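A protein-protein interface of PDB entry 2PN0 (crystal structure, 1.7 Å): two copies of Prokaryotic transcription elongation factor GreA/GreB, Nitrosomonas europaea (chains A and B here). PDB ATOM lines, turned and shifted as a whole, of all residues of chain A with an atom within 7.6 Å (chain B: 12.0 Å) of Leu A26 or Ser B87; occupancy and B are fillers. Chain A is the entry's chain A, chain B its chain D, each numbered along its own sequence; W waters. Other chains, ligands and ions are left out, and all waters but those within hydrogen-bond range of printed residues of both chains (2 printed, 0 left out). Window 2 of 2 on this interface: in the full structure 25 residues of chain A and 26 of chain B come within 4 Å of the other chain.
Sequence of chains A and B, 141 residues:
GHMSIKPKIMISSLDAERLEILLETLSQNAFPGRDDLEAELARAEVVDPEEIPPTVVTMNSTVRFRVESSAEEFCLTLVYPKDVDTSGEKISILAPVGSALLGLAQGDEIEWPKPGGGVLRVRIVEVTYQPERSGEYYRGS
Ser B87 touches Leu A26. CB of Asn A29 touches O of Ser B87 (3.8 Å). ND2 of Asn A29 touches OE2 of Glu B89 (3.5 Å). Phe B74 touches Ala A30 (CB to O, 3.3 Å). Phe A31 touches Gly B88 (CB to O, 3.8 Å). CB of Pro A81 touches O of Thr B86, at 3.4 Å. C of Ser B87 touches CD1 of Leu A94, 3.9 Å away. Gly B88 touches Leu A94 (N to CD1, 3.9 Å).
The side-chain carboxylate of Asp B85 is in hydrogen-bond range of the backbone NH of Ser B87. O of Asn A29 lies within hydrogen-bond range of NH1 of Arg A34 (3.0 Å). The backbone carbonyl oxygen (O) of Glu B89 is in hydrogen-bond range of the backbone NH (N) of Thr B77. The backbone carbonyl oxygen of Leu A26 lies within hydrogen-bond range of the guanidinium group of Arg A34 (2.8 Å). N of Leu A94 lies within hydrogen-bond range of OG of Ser A92 (2.9 Å).
Water W1 bridges the backbone carbonyl oxygen of Gly B88 (2.8 Å) and the backbone carbonyl oxygen of Leu A94 (2.8 Å). Water W2 bridges O of Ala A30 (2.8 Å) and N of OCS B75 (3.0 Å).
Of the 17 printed residues of chain A, 6 touch a printed residue of chain B. Hydrophobic or aromatic side chains of chain A that line the printed part of chain B: Leu A26, Phe A31, Pro A81 and Leu A94. Of the 18 printed residues of chain B, 5 touch a printed residue of chain A. Printed residues of chain B that touch a printed residue of chain A: Phe B74, Thr B86, Ser B87, Gly B88 and Glu B89. Among the printed residues, no Asp or Glu carboxylate lies within 4 Å of a Lys or Arg side-chain nitrogen of the other chain.
Leu A26 touches one residue of chain B. Printed residues of chain A within 4 Å of Ser B87: Leu A26 (3.4 Å), Asn A29 (3.8 Å) and Leu A94 (3.9 Å). No residue of chain B comes within 4 Å of Leu A22. No residue of chain B comes within 4 Å of Thr A25. Ala A30 touches just one residue of chain B: Phe B74. Leu A94 touches two residues of chain B. Of the printed residues of chain A, Thr B86 touches Pro A81 (3.4 Å). Of the printed residues of chain B, Asn A29 touches Ser B87 (3.8 Å) and Glu B89 (3.5 Å). Of the printed residues of chain A, Glu B89 touches Asn A29 (3.5 Å). Arg A34 touches none of the printed residues of chain B. OCS B75 touches none of the printed residues of chain A. The nearest residue of chain A that does not touch Ser B87 is Phe A31 (5.1 Å).
2 positions are printed for both chains. Of the 8 pairs that touch across the chains among the printed residues, none has its exchanged pair printed and touching as well.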
ATOM      1  N   GLU A  20     -15.964 -20.284   7.395  1.00  0.00           N
ATOM      2  CA  GLU A  20     -15.936 -20.909   8.714  1.00  0.00           C
ATOM      3  C   GLU A  20     -17.337 -20.900   9.317  1.00  0.00           C
ATOM      4  O   GLU A  20     -17.785 -21.910   9.872  1.00  0.00           O
ATOM      5  CB  GLU A  20     -14.929 -20.229   9.652  1.00  0.00           C
ATOM      6  CG  GLU A  20     -14.981 -20.731  11.108  1.00  0.00           C
ATOM      7  CD  GLU A  20     -14.471 -22.161  11.298  1.00  0.00           C
ATOM      8  OE1 GLU A  20     -13.820 -22.709  10.377  1.00  0.00           O
ATOM      9  OE2 GLU A  20     -14.722 -22.750  12.384  1.00  0.00           O
ATOM     10  N   ILE A  21     -18.041 -19.773   9.199  1.00  0.00           N
ATOM     11  CA  ILE A  21     -19.393 -19.666   9.768  1.00  0.00           C
ATOM     12  C   ILE A  21     -20.331 -20.592   8.998  1.00  0.00           C
ATOM     13  O   ILE A  21     -21.187 -21.269   9.583  1.00  0.00           O
ATOM     14  CB  ILE A  21     -19.920 -18.221   9.722  1.00  0.00           C
ATOM     15  CG1 ILE A  21     -19.093 -17.313  10.660  1.00  0.00           C
ATOM     16  CG2 ILE A  21     -21.456 -18.165  10.065  1.00  0.00           C
ATOM     17  CD1 ILE A  21     -19.313 -15.839  10.428  1.00  0.00           C
ATOM     18  N   LEU A  22     -20.158 -20.643   7.687  1.00  0.00           N
ATOM     19  CA  LEU A  22     -20.974 -21.564   6.886  1.00  0.00           C
ATOM     20  C   LEU A  22     -20.815 -23.000   7.373  1.00  0.00           C
ATOM     21  O   LEU A  22     -21.800 -23.739   7.527  1.00  0.00           O
ATOM     22  CB  LEU A  22     -20.620 -21.447   5.392  1.00  0.00           C
ATOM     23  CG  LEU A  22     -21.411 -22.356   4.456  1.00  0.00           C
ATOM     24  CD1 LEU A  22     -22.945 -22.142   4.504  1.00  0.00           C
ATOM     25  CD2 LEU A  22     -20.854 -22.281   3.018  1.00  0.00           C
ATOM     26  N   LEU A  23     -19.572 -23.428   7.584  1.00  0.00           N
ATOM     27  CA  LEU A  23     -19.306 -24.817   7.896  1.00  0.00           C
ATOM     28  C   LEU A  23     -19.790 -25.146   9.324  1.00  0.00           C
ATOM     29  O   LEU A  23     -20.205 -26.278   9.590  1.00  0.00           O
ATOM     30  CB  LEU A  23     -17.808 -25.080   7.760  1.00  0.00           C
ATOM     31  CG  LEU A  23     -17.321 -25.059   6.312  1.00  0.00           C
ATOM     32  CD1 LEU A  23     -15.781 -25.092   6.334  1.00  0.00           C
ATOM     33  CD2 LEU A  23     -17.884 -26.254   5.555  1.00  0.00           C
ATOM     34  N   GLU A  24     -19.700 -24.159  10.222  1.00  0.00           N
ATOM     35  CA  GLU A  24     -20.204 -24.262  11.591  1.00  0.00           C
ATOM     36  C   GLU A  24     -21.728 -24.378  11.579  1.00  0.00           C
ATOM     37  O   GLU A  24     -22.318 -25.124  12.361  1.00  0.00           O
ATOM     38  CB  GLU A  24     -19.798 -23.021  12.390  1.00  0.00           C
ATOM     39  CG  GLU A  24     -18.333 -23.023  12.811  1.00  0.00           C
ATOM     40  CD  GLU A  24     -17.885 -21.757  13.523  1.00  0.00           C
ATOM     41  OE1 GLU A  24     -18.741 -20.891  13.840  1.00  0.00           O
ATOM     42  OE2 GLU A  24     -16.659 -21.634  13.772  1.00  0.00           O
ATOM     43  N   THR A  25     -22.365 -23.609  10.696  1.00  0.00           N
ATOM     44  CA  THR A  25     -23.827 -23.607  10.644  1.00  0.00           C
ATOM     45  C   THR A  25     -24.345 -24.963  10.161  1.00  0.00           C
ATOM     46  O   THR A  25     -25.346 -25.483  10.693  1.00  0.00           O
ATOM     47  CB  THR A  25     -24.365 -22.460   9.766  1.00  0.00           C
ATOM     48  OG1 THR A  25     -23.920 -21.202  10.307  1.00  0.00           O
ATOM     49  CG2 THR A  25     -25.897 -22.478   9.737  1.00  0.00           C
ATOM     50  N   LEU A  26     -23.652 -25.522   9.164  1.00  0.00           N
ATOM     51  CA  LEU A  26     -23.948 -26.850   8.622  1.00  0.00           C
ATOM     52  C   LEU A  26     -23.198 -27.958   9.353  1.00  0.00           C
ATOM     53  O   LEU A  26     -22.796 -28.942   8.738  1.00  0.00           O
ATOM     54  CB  LEU A  26     -23.556 -26.912   7.142  1.00  0.00           C
ATOM     55  CG  LEU A  26     -24.400 -25.989   6.245  1.00  0.00           C
ATOM     56  CD1 LEU A  26     -23.959 -26.026   4.814  1.00  0.00           C
ATOM     57  CD2 LEU A  26     -25.912 -26.315   6.393  1.00  0.00           C
ATOM     58  N   SER A  27     -23.017 -27.840  10.660  1.00  0.00           N
ATOM     59  CA  SER A  27     -22.110 -28.732  11.400  1.00  0.00           C
ATOM     60  C   SER A  27     -22.347 -30.224  11.129  1.00  0.00           C
ATOM     61  O   SER A  27     -21.394 -31.028  11.071  1.00  0.00           O
ATOM     62  CB  SER A  27     -22.195 -28.438  12.903  1.00  0.00           C
ATOM     63  OG  SER A  27     -23.530 -28.162  13.317  1.00  0.00           O
ATOM     64  N   GLN A  28     -23.627 -30.588  10.984  1.00  0.00           N
ATOM     65  CA  GLN A  28     -24.056 -31.982  10.811  1.00  0.00           C
ATOM     66  C   GLN A  28     -24.117 -32.433   9.365  1.00  0.00           C
ATOM     67  O   GLN A  28     -24.475 -33.583   9.088  1.00  0.00           O
ATOM     68  CB  GLN A  28     -25.430 -32.221  11.449  1.00  0.00           C
ATOM     69  CG  GLN A  28     -25.416 -32.313  12.970  1.00  0.00           C
ATOM     70  CD  GLN A  28     -26.444 -33.297  13.513  1.00  0.00           C
ATOM     71  OE1 GLN A  28     -26.929 -34.175  12.794  1.00  0.00           O
ATOM     72  NE2 GLN A  28     -26.773 -33.161  14.796  1.00  0.00           N
ATOM     73  N   ASN A  29     -23.810 -31.537   8.432  1.00  0.00           N
ATOM     74  CA  ASN A  29     -23.930 -31.894   7.012  1.00  0.00           C
ATOM     75  C   ASN A  29     -22.636 -32.471   6.425  1.00  0.00           C
ATOM     76  O   ASN A  29     -21.711 -31.742   6.073  1.00  0.00           O
ATOM     77  CB  ASN A  29     -24.498 -30.719   6.204  1.00  0.00           C
ATOM     78  CG  ASN A  29     -25.938 -30.376   6.629  1.00  0.00           C
ATOM     79  OD1 ASN A  29     -26.175 -29.414   7.378  1.00  0.00           O
ATOM     80  ND2 ASN A  29     -26.896 -31.200   6.197  1.00  0.00           N
ATOM     81  N   ALA A  30     -22.580 -33.799   6.347  1.00  0.00           N
ATOM     82  CA  ALA A  30     -21.380 -34.483   5.889  1.00  0.00           C
ATOM     83  C   ALA A  30     -21.371 -34.550   4.363  1.00  0.00           C
ATOM     84  O   ALA A  30     -21.652 -35.602   3.768  1.00  0.00           O
ATOM     85  CB  ALA A  30     -21.292 -35.886   6.515  1.00  0.00           C
ATOM     86  N   PHE A  31     -21.052 -33.426   3.723  1.00  0.00           N
ATOM     87  CA  PHE A  31     -21.055 -33.353   2.248  1.00  0.00           C
ATOM     88  C   PHE A  31     -19.715 -33.903   1.715  1.00  0.00           C
ATOM     89  O   PHE A  31     -18.699 -33.897   2.443  1.00  0.00           O
ATOM     90  CB  PHE A  31     -21.354 -31.935   1.724  1.00  0.00           C
ATOM     91  CG  PHE A  31     -20.353 -30.876   2.178  1.00  0.00           C
ATOM     92  CD1 PHE A  31     -19.185 -30.647   1.470  1.00  0.00           C
ATOM     93  CD2 PHE A  31     -20.599 -30.124   3.323  1.00  0.00           C
ATOM     94  CE1 PHE A  31     -18.277 -29.677   1.881  1.00  0.00           C
ATOM     95  CE2 PHE A  31     -19.681 -29.148   3.743  1.00  0.00           C
ATOM     96  CZ  PHE A  31     -18.526 -28.940   3.016  1.00  0.00           C
ATOM     97  N   ARG A  34     -15.884 -32.669   2.524  1.00  0.00           N
ATOM     98  CA  ARG A  34     -15.898 -31.672   3.609  1.00  0.00           C
ATOM     99  C   ARG A  34     -14.621 -31.686   4.411  1.00  0.00           C
ATOM    100  O   ARG A  34     -14.031 -30.617   4.685  1.00  0.00           O
ATOM    101  CB  ARG A  34     -17.072 -31.921   4.554  1.00  0.00           C
ATOM    102  CG  ARG A  34     -17.069 -31.020   5.788  1.00  0.00           C
ATOM    103  CD  ARG A  34     -18.284 -31.262   6.653  1.00  0.00           C
ATOM    104  NE  ARG A  34     -18.225 -30.310   7.748  1.00  0.00           N
ATOM    105  CZ  ARG A  34     -19.173 -29.433   8.085  1.00  0.00           C
ATOM    106  NH1 ARG A  34     -20.351 -29.416   7.464  1.00  0.00           N
ATOM    107  NH2 ARG A  34     -18.941 -28.600   9.101  1.00  0.00           N
ATOM    108  N   GLU A  38     -12.223 -28.491   4.783  1.00  0.00           N
ATOM    109  CA  GLU A  38     -11.869 -27.962   6.122  1.00  0.00           C
ATOM    110  C   GLU A  38     -10.352 -27.913   6.347  1.00  0.00           C
ATOM    111  O   GLU A  38      -9.791 -26.905   6.840  1.00  0.00           O
ATOM    112  CB  GLU A  38     -12.521 -28.834   7.220  1.00  0.00           C
ATOM    113  CG  GLU A  38     -13.997 -28.637   7.313  1.00  0.00           C
ATOM    114  CD  GLU A  38     -14.683 -29.544   8.340  1.00  0.00           C
ATOM    115  OE1 GLU A  38     -14.149 -30.649   8.661  1.00  0.00           O
ATOM    116  OE2 GLU A  38     -15.793 -29.149   8.792  1.00  0.00           O
ATOM    117  N   PRO A  81     -23.836 -20.841  -1.113  1.00  0.00           N
ATOM    118  CA  PRO A  81     -25.148 -21.465  -1.383  1.00  0.00           C
ATOM    119  C   PRO A  81     -26.263 -20.472  -1.762  1.00  0.00           C
ATOM    120  O   PRO A  81     -27.033 -20.769  -2.681  1.00  0.00           O
ATOM    121  CB  PRO A  81     -25.447 -22.223  -0.094  1.00  0.00           C
ATOM    122  CG  PRO A  81     -24.089 -22.661   0.362  1.00  0.00           C
ATOM    123  CD  PRO A  81     -23.211 -21.430   0.089  1.00  0.00           C
ATOM    124  N   SER A  92     -21.897 -24.106  -6.338  1.00  0.00           N
ATOM    125  CA  SER A  92     -21.673 -23.907  -4.891  1.00  0.00           C
ATOM    126  C   SER A  92     -20.296 -24.405  -4.436  1.00  0.00           C
ATOM    127  O   SER A  92     -19.834 -25.472  -4.871  1.00  0.00           O
ATOM    128  CB  SER A  92     -22.773 -24.612  -4.066  1.00  0.00           C
ATOM    129  OG  SER A  92     -22.565 -24.509  -2.669  1.00  0.00           O
ATOM    130  N   LEU A  94     -20.098 -25.887  -1.829  1.00  0.00           N
ATOM    131  CA  LEU A  94     -20.464 -27.207  -1.186  1.00  0.00           C
ATOM    132  C   LEU A  94     -20.575 -28.357  -2.186  1.00  0.00           C
ATOM    133  O   LEU A  94     -20.638 -29.514  -1.780  1.00  0.00           O
ATOM    134  CB  LEU A  94     -21.780 -27.119  -0.387  1.00  0.00           C
ATOM    135  CG  LEU A  94     -21.837 -25.964   0.619  1.00  0.00           C
ATOM    136  CD1 LEU A  94     -23.150 -26.129   1.387  1.00  0.00           C
ATOM    137  CD2 LEU A  94     -20.662 -26.016   1.560  1.00  0.00           C
ATOM    138  N   GLU B  73     -19.010 -42.375   4.261  1.00  0.00           N
ATOM    139  CA  GLU B  73     -20.186 -42.333   3.359  1.00  0.00           C
ATOM    140  C   GLU B  73     -20.842 -40.942   3.328  1.00  0.00           C
ATOM    141  O   GLU B  73     -20.726 -40.157   4.254  1.00  0.00           O
ATOM    142  CB  GLU B  73     -21.207 -43.395   3.777  1.00  0.00           C
ATOM    143  CG  GLU B  73     -20.686 -44.834   3.648  1.00  0.00           C
ATOM    144  CD  GLU B  73     -21.760 -45.901   3.884  1.00  0.00           C
ATOM    145  OE1 GLU B  73     -22.859 -45.574   4.394  1.00  0.00           O
ATOM    146  OE2 GLU B  73     -21.509 -47.079   3.530  1.00  0.00           O
ATOM    147  N   PHE B  74     -21.534 -40.644   2.237  1.00  0.00           N
ATOM    148  CA  PHE B  74     -22.326 -39.434   2.158  1.00  0.00           C
ATOM    149  C   PHE B  74     -23.397 -39.700   1.097  1.00  0.00           C
ATOM    150  O   PHE B  74     -23.322 -40.684   0.344  1.00  0.00           O
ATOM    151  CB  PHE B  74     -21.474 -38.236   1.729  1.00  0.00           C
ATOM    152  CG  PHE B  74     -20.757 -38.454   0.405  1.00  0.00           C
ATOM    153  CD1 PHE B  74     -21.391 -38.159  -0.817  1.00  0.00           C
ATOM    154  CD2 PHE B  74     -19.466 -38.957   0.371  1.00  0.00           C
ATOM    155  CE1 PHE B  74     -20.715 -38.376  -2.045  1.00  0.00           C
ATOM    156  CE2 PHE B  74     -18.790 -39.191  -0.858  1.00  0.00           C
ATOM    157  CZ  PHE B  74     -19.423 -38.893  -2.072  1.00  0.00           C
ATOM    158  N   OCS B  75     -24.363 -38.798   1.056  1.00  0.00           N
ATOM    159  CA  OCS B  75     -25.488 -38.957   0.132  1.00  0.00           C
ATOM    160  CB  OCS B  75     -26.798 -39.020   0.903  1.00  0.00           C
ATOM    161  SG  OCS B  75     -26.966 -40.551   1.801  1.00  0.00           S
ATOM    162  C   OCS B  75     -25.582 -37.747  -0.768  1.00  0.00           C
ATOM    163  O   OCS B  75     -25.248 -36.635  -0.342  1.00  0.00           O
ATOM    164  OD1 OCS B  75     -28.351 -40.675   2.158  1.00  0.00           O
ATOM    165  OD2 OCS B  75     -26.125 -40.502   2.949  1.00  0.00           O
ATOM    166  OD3 OCS B  75     -26.616 -41.603   1.000  1.00  0.00           O
ATOM    167  N   LEU B  76     -26.081 -37.964  -1.980  1.00  0.00           N
ATOM    168  CA  LEU B  76     -26.534 -36.882  -2.854  1.00  0.00           C
ATOM    169  C   LEU B  76     -27.855 -37.282  -3.501  1.00  0.00           C
ATOM    170  O   LEU B  76     -27.985 -38.409  -3.946  1.00  0.00           O
ATOM    171  CB  LEU B  76     -25.565 -36.635  -4.010  1.00  0.00           C
ATOM    172  CG  LEU B  76     -24.186 -36.102  -3.611  1.00  0.00           C
ATOM    173  CD1 LEU B  76     -23.291 -36.188  -4.830  1.00  0.00           C
ATOM    174  CD2 LEU B  76     -24.223 -34.634  -3.029  1.00  0.00           C
ATOM    175  N   THR B  77     -28.786 -36.335  -3.552  1.00  0.00           N
ATOM    176  CA  THR B  77     -30.061 -36.535  -4.191  1.00  0.00           C
ATOM    177  C   THR B  77     -30.068 -35.825  -5.558  1.00  0.00           C
ATOM    178  O   THR B  77     -29.849 -34.616  -5.638  1.00  0.00           O
ATOM    179  CB  THR B  77     -31.212 -36.054  -3.311  1.00  0.00           C
ATOM    180  OG1 THR B  77     -31.189 -36.820  -2.091  1.00  0.00           O
ATOM    181  CG2 THR B  77     -32.509 -36.265  -4.029  1.00  0.00           C
ATOM    182  N   VAL B  79     -31.448 -34.111  -8.689  1.00  0.00           N
ATOM    183  CA  VAL B  79     -32.665 -33.327  -8.888  1.00  0.00           C
ATOM    184  C   VAL B  79     -32.660 -32.454 -10.138  1.00  0.00           C
ATOM    185  O   VAL B  79     -31.598 -32.222 -10.767  1.00  0.00           O
ATOM    186  CB  VAL B  79     -32.931 -32.412  -7.643  1.00  0.00           C
ATOM    187  CG1 VAL B  79     -33.127 -33.253  -6.343  1.00  0.00           C
ATOM    188  CG2 VAL B  79     -31.784 -31.406  -7.483  1.00  0.00           C
ATOM    189  N   PRO B  81     -33.130 -28.718 -11.872  1.00  0.00           N
ATOM    190  CA  PRO B  81     -32.442 -27.488 -11.448  1.00  0.00           C
ATOM    191  C   PRO B  81     -33.149 -26.651 -10.376  1.00  0.00           C
ATOM    192  O   PRO B  81     -32.489 -26.110  -9.495  1.00  0.00           O
ATOM    193  CB  PRO B  81     -32.321 -26.711 -12.755  1.00  0.00           C
ATOM    194  CG  PRO B  81     -32.166 -27.797 -13.775  1.00  0.00           C
ATOM    195  CD  PRO B  81     -33.150 -28.830 -13.343  1.00  0.00           C
ATOM    196  N   LYS B  82     -34.472 -26.611 -10.422  1.00  0.00           N
ATOM    197  CA  LYS B  82     -35.265 -25.769  -9.524  1.00  0.00           C
ATOM    198  C   LYS B  82     -35.369 -26.334  -8.115  1.00  0.00           C
ATOM    199  O   LYS B  82     -35.736 -25.598  -7.183  1.00  0.00           O
ATOM    200  CB  LYS B  82     -36.654 -25.588 -10.117  1.00  0.00           C
ATOM    201  CG  LYS B  82     -36.686 -24.591 -11.275  1.00  0.00           C
ATOM    202  CD  LYS B  82     -38.097 -24.465 -11.850  1.00  0.00           C
ATOM    203  CE  LYS B  82     -38.117 -23.605 -13.123  1.00  0.00           C
ATOM    204  NZ  LYS B  82     -39.488 -23.141 -13.443  1.00  0.00           N
ATOM    205  N   ASP B  83     -35.039 -27.626  -7.972  1.00  0.00           N
ATOM    206  CA  ASP B  83     -35.212 -28.376  -6.728  1.00  0.00           C
ATOM    207  C   ASP B  83     -33.957 -28.523  -5.860  1.00  0.00           C
ATOM    208  O   ASP B  83     -33.978 -29.179  -4.801  1.00  0.00           O
ATOM    209  CB  ASP B  83     -35.849 -29.728  -7.028  1.00  0.00           C
ATOM    210  CG  ASP B  83     -37.280 -29.593  -7.557  1.00  0.00           C
ATOM    211  OD1 ASP B  83     -37.958 -28.563  -7.249  1.00  0.00           O
ATOM    212  OD2 ASP B  83     -37.733 -30.506  -8.273  1.00  0.00           O
ATOM    213  N   VAL B  84     -32.861 -27.907  -6.301  1.00  0.00           N
ATOM    214  CA  VAL B  84     -31.628 -27.986  -5.557  1.00  0.00           C
ATOM    215  C   VAL B  84     -31.824 -27.228  -4.243  1.00  0.00           C
ATOM    216  O   VAL B  84     -32.531 -26.219  -4.222  1.00  0.00           O
ATOM    217  CB  VAL B  84     -30.450 -27.400  -6.359  1.00  0.00           C
ATOM    218  CG1 VAL B  84     -30.630 -25.903  -6.589  1.00  0.00           C
ATOM    219  CG2 VAL B  84     -29.140 -27.695  -5.670  1.00  0.00           C
ATOM    220  N   ASP B  85     -31.213 -27.751  -3.172  1.00  0.00           N
ATOM    221  CA  ASP B  85     -31.209 -27.146  -1.829  1.00  0.00           C
ATOM    222  C   ASP B  85     -29.917 -26.342  -1.673  1.00  0.00           C
ATOM    223  O   ASP B  85     -29.155 -26.237  -2.619  1.00  0.00           O
ATOM    224  CB  ASP B  85     -31.292 -28.228  -0.729  1.00  0.00           C
ATOM    225  CG  ASP B  85     -29.959 -29.003  -0.514  1.00  0.00           C
ATOM    226  OD1 ASP B  85     -29.114 -29.098  -1.449  1.00  0.00           O
ATOM    227  OD2 ASP B  85     -29.756 -29.538   0.604  1.00  0.00           O
ATOM    228  N   THR B  86     -29.684 -25.794  -0.478  1.00  0.00           N
ATOM    229  CA  THR B  86     -28.544 -24.926  -0.187  1.00  0.00           C
ATOM    230  C   THR B  86     -27.651 -25.521   0.935  1.00  0.00           C
ATOM    231  O   THR B  86     -26.955 -24.766   1.657  1.00  0.00           O
ATOM    232  CB  THR B  86     -29.028 -23.539   0.363  1.00  0.00           C
ATOM    233  OG1 THR B  86     -30.171 -23.727   1.204  1.00  0.00           O
ATOM    234  CG2 THR B  86     -29.368 -22.556  -0.736  1.00  0.00           C
ATOM    235  N   SER B  87     -27.713 -26.837   1.140  1.00  0.00           N
ATOM    236  CA  SER B  87     -26.971 -27.441   2.254  1.00  0.00           C
ATOM    237  C   SER B  87     -26.077 -28.644   1.933  1.00  0.00           C
ATOM    238  O   SER B  87     -25.622 -29.388   2.828  1.00  0.00           O
ATOM    239  CB  SER B  87     -27.904 -27.695   3.443  1.00  0.00           C
ATOM    240  OG  SER B  87     -28.280 -26.445   4.000  1.00  0.00           O
ATOM    241  N   GLY B  88     -25.837 -28.822   0.642  1.00  0.00           N
ATOM    242  CA  GLY B  88     -24.844 -29.772   0.176  1.00  0.00           C
ATOM    243  C   GLY B  88     -25.372 -31.168  -0.091  1.00  0.00           C
ATOM    244  O   GLY B  88     -24.559 -32.051  -0.388  1.00  0.00           O
ATOM    245  N   GLU B  89     -26.705 -31.351  -0.038  1.00  0.00           N
ATOM    246  CA  GLU B  89     -27.343 -32.678  -0.083  1.00  0.00           C
ATOM    247  C   GLU B  89     -27.930 -33.005  -1.452  1.00  0.00           C
ATOM    248  O   GLU B  89     -28.163 -34.174  -1.760  1.00  0.00           O
ATOM    249  CB  GLU B  89     -28.490 -32.779   0.934  1.00  0.00           C
ATOM    250  CG  GLU B  89     -28.099 -32.539   2.387  1.00  0.00           C
ATOM    251  CD  GLU B  89     -29.263 -32.776   3.338  1.00  0.00           C
ATOM    252  OE1 GLU B  89     -30.415 -32.392   2.996  1.00  0.00           O
ATOM    253  OE2 GLU B  89     -29.021 -33.346   4.422  1.00  0.00           O
ATOM    254  N   LYS B  90     -28.212 -31.965  -2.245  1.00  0.00           N
ATOM    255  CA  LYS B  90     -28.869 -32.155  -3.532  1.00  0.00           C
ATOM    256  C   LYS B  90     -27.921 -31.740  -4.650  1.00  0.00           C
ATOM    257  O   LYS B  90     -27.029 -30.910  -4.448  1.00  0.00           O
ATOM    258  CB  LYS B  90     -30.187 -31.398  -3.598  1.00  0.00           C
ATOM    259  CG  LYS B  90     -31.219 -32.008  -2.629  1.00  0.00           C
ATOM    260  CD  LYS B  90     -32.562 -31.343  -2.671  1.00  0.00           C
ATOM    261  CE  LYS B  90     -33.360 -31.801  -1.449  1.00  0.00           C
ATOM    262  NZ  LYS B  90     -34.618 -31.024  -1.346  1.00  0.00           N
ATOM    263  N   ILE B  91     -28.071 -32.375  -5.801  1.00  0.00           N
ATOM    264  CA  ILE B  91     -27.193 -32.059  -6.921  1.00  0.00           C
ATOM    265  C   ILE B  91     -28.003 -32.013  -8.222  1.00  0.00           C
ATOM    266  O   ILE B  91     -28.814 -32.922  -8.498  1.00  0.00           O
ATOM    267  CB  ILE B  91     -26.006 -33.047  -6.990  1.00  0.00           C
ATOM    268  CG1 ILE B  91     -24.913 -32.511  -7.964  1.00  0.00           C
ATOM    269  CG2 ILE B  91     -26.491 -34.483  -7.356  1.00  0.00           C
ATOM    270  CD1 ILE B  91     -23.574 -33.331  -7.940  1.00  0.00           C
ATOM    271  N   SER B  92     -27.812 -30.950  -9.007  1.00  0.00           N
ATOM    272  CA  SER B  92     -28.557 -30.793 -10.261  1.00  0.00           C
ATOM    273  C   SER B  92     -28.114 -31.792 -11.333  1.00  0.00           C
ATOM    274  O   SER B  92     -26.915 -32.070 -11.449  1.00  0.00           O
ATOM    275  CB  SER B  92     -28.440 -29.351 -10.794  1.00  0.00           C
ATOM    276  OG  SER B  92     -29.098 -29.247 -12.025  1.00  0.00           O
HETATM  277  O   HOH W   1     -22.510 -31.531  -2.191  1.00  0.00           O
HETATM  278  O   HOH W   2     -24.136 -36.828   3.292  1.00  0.00           O
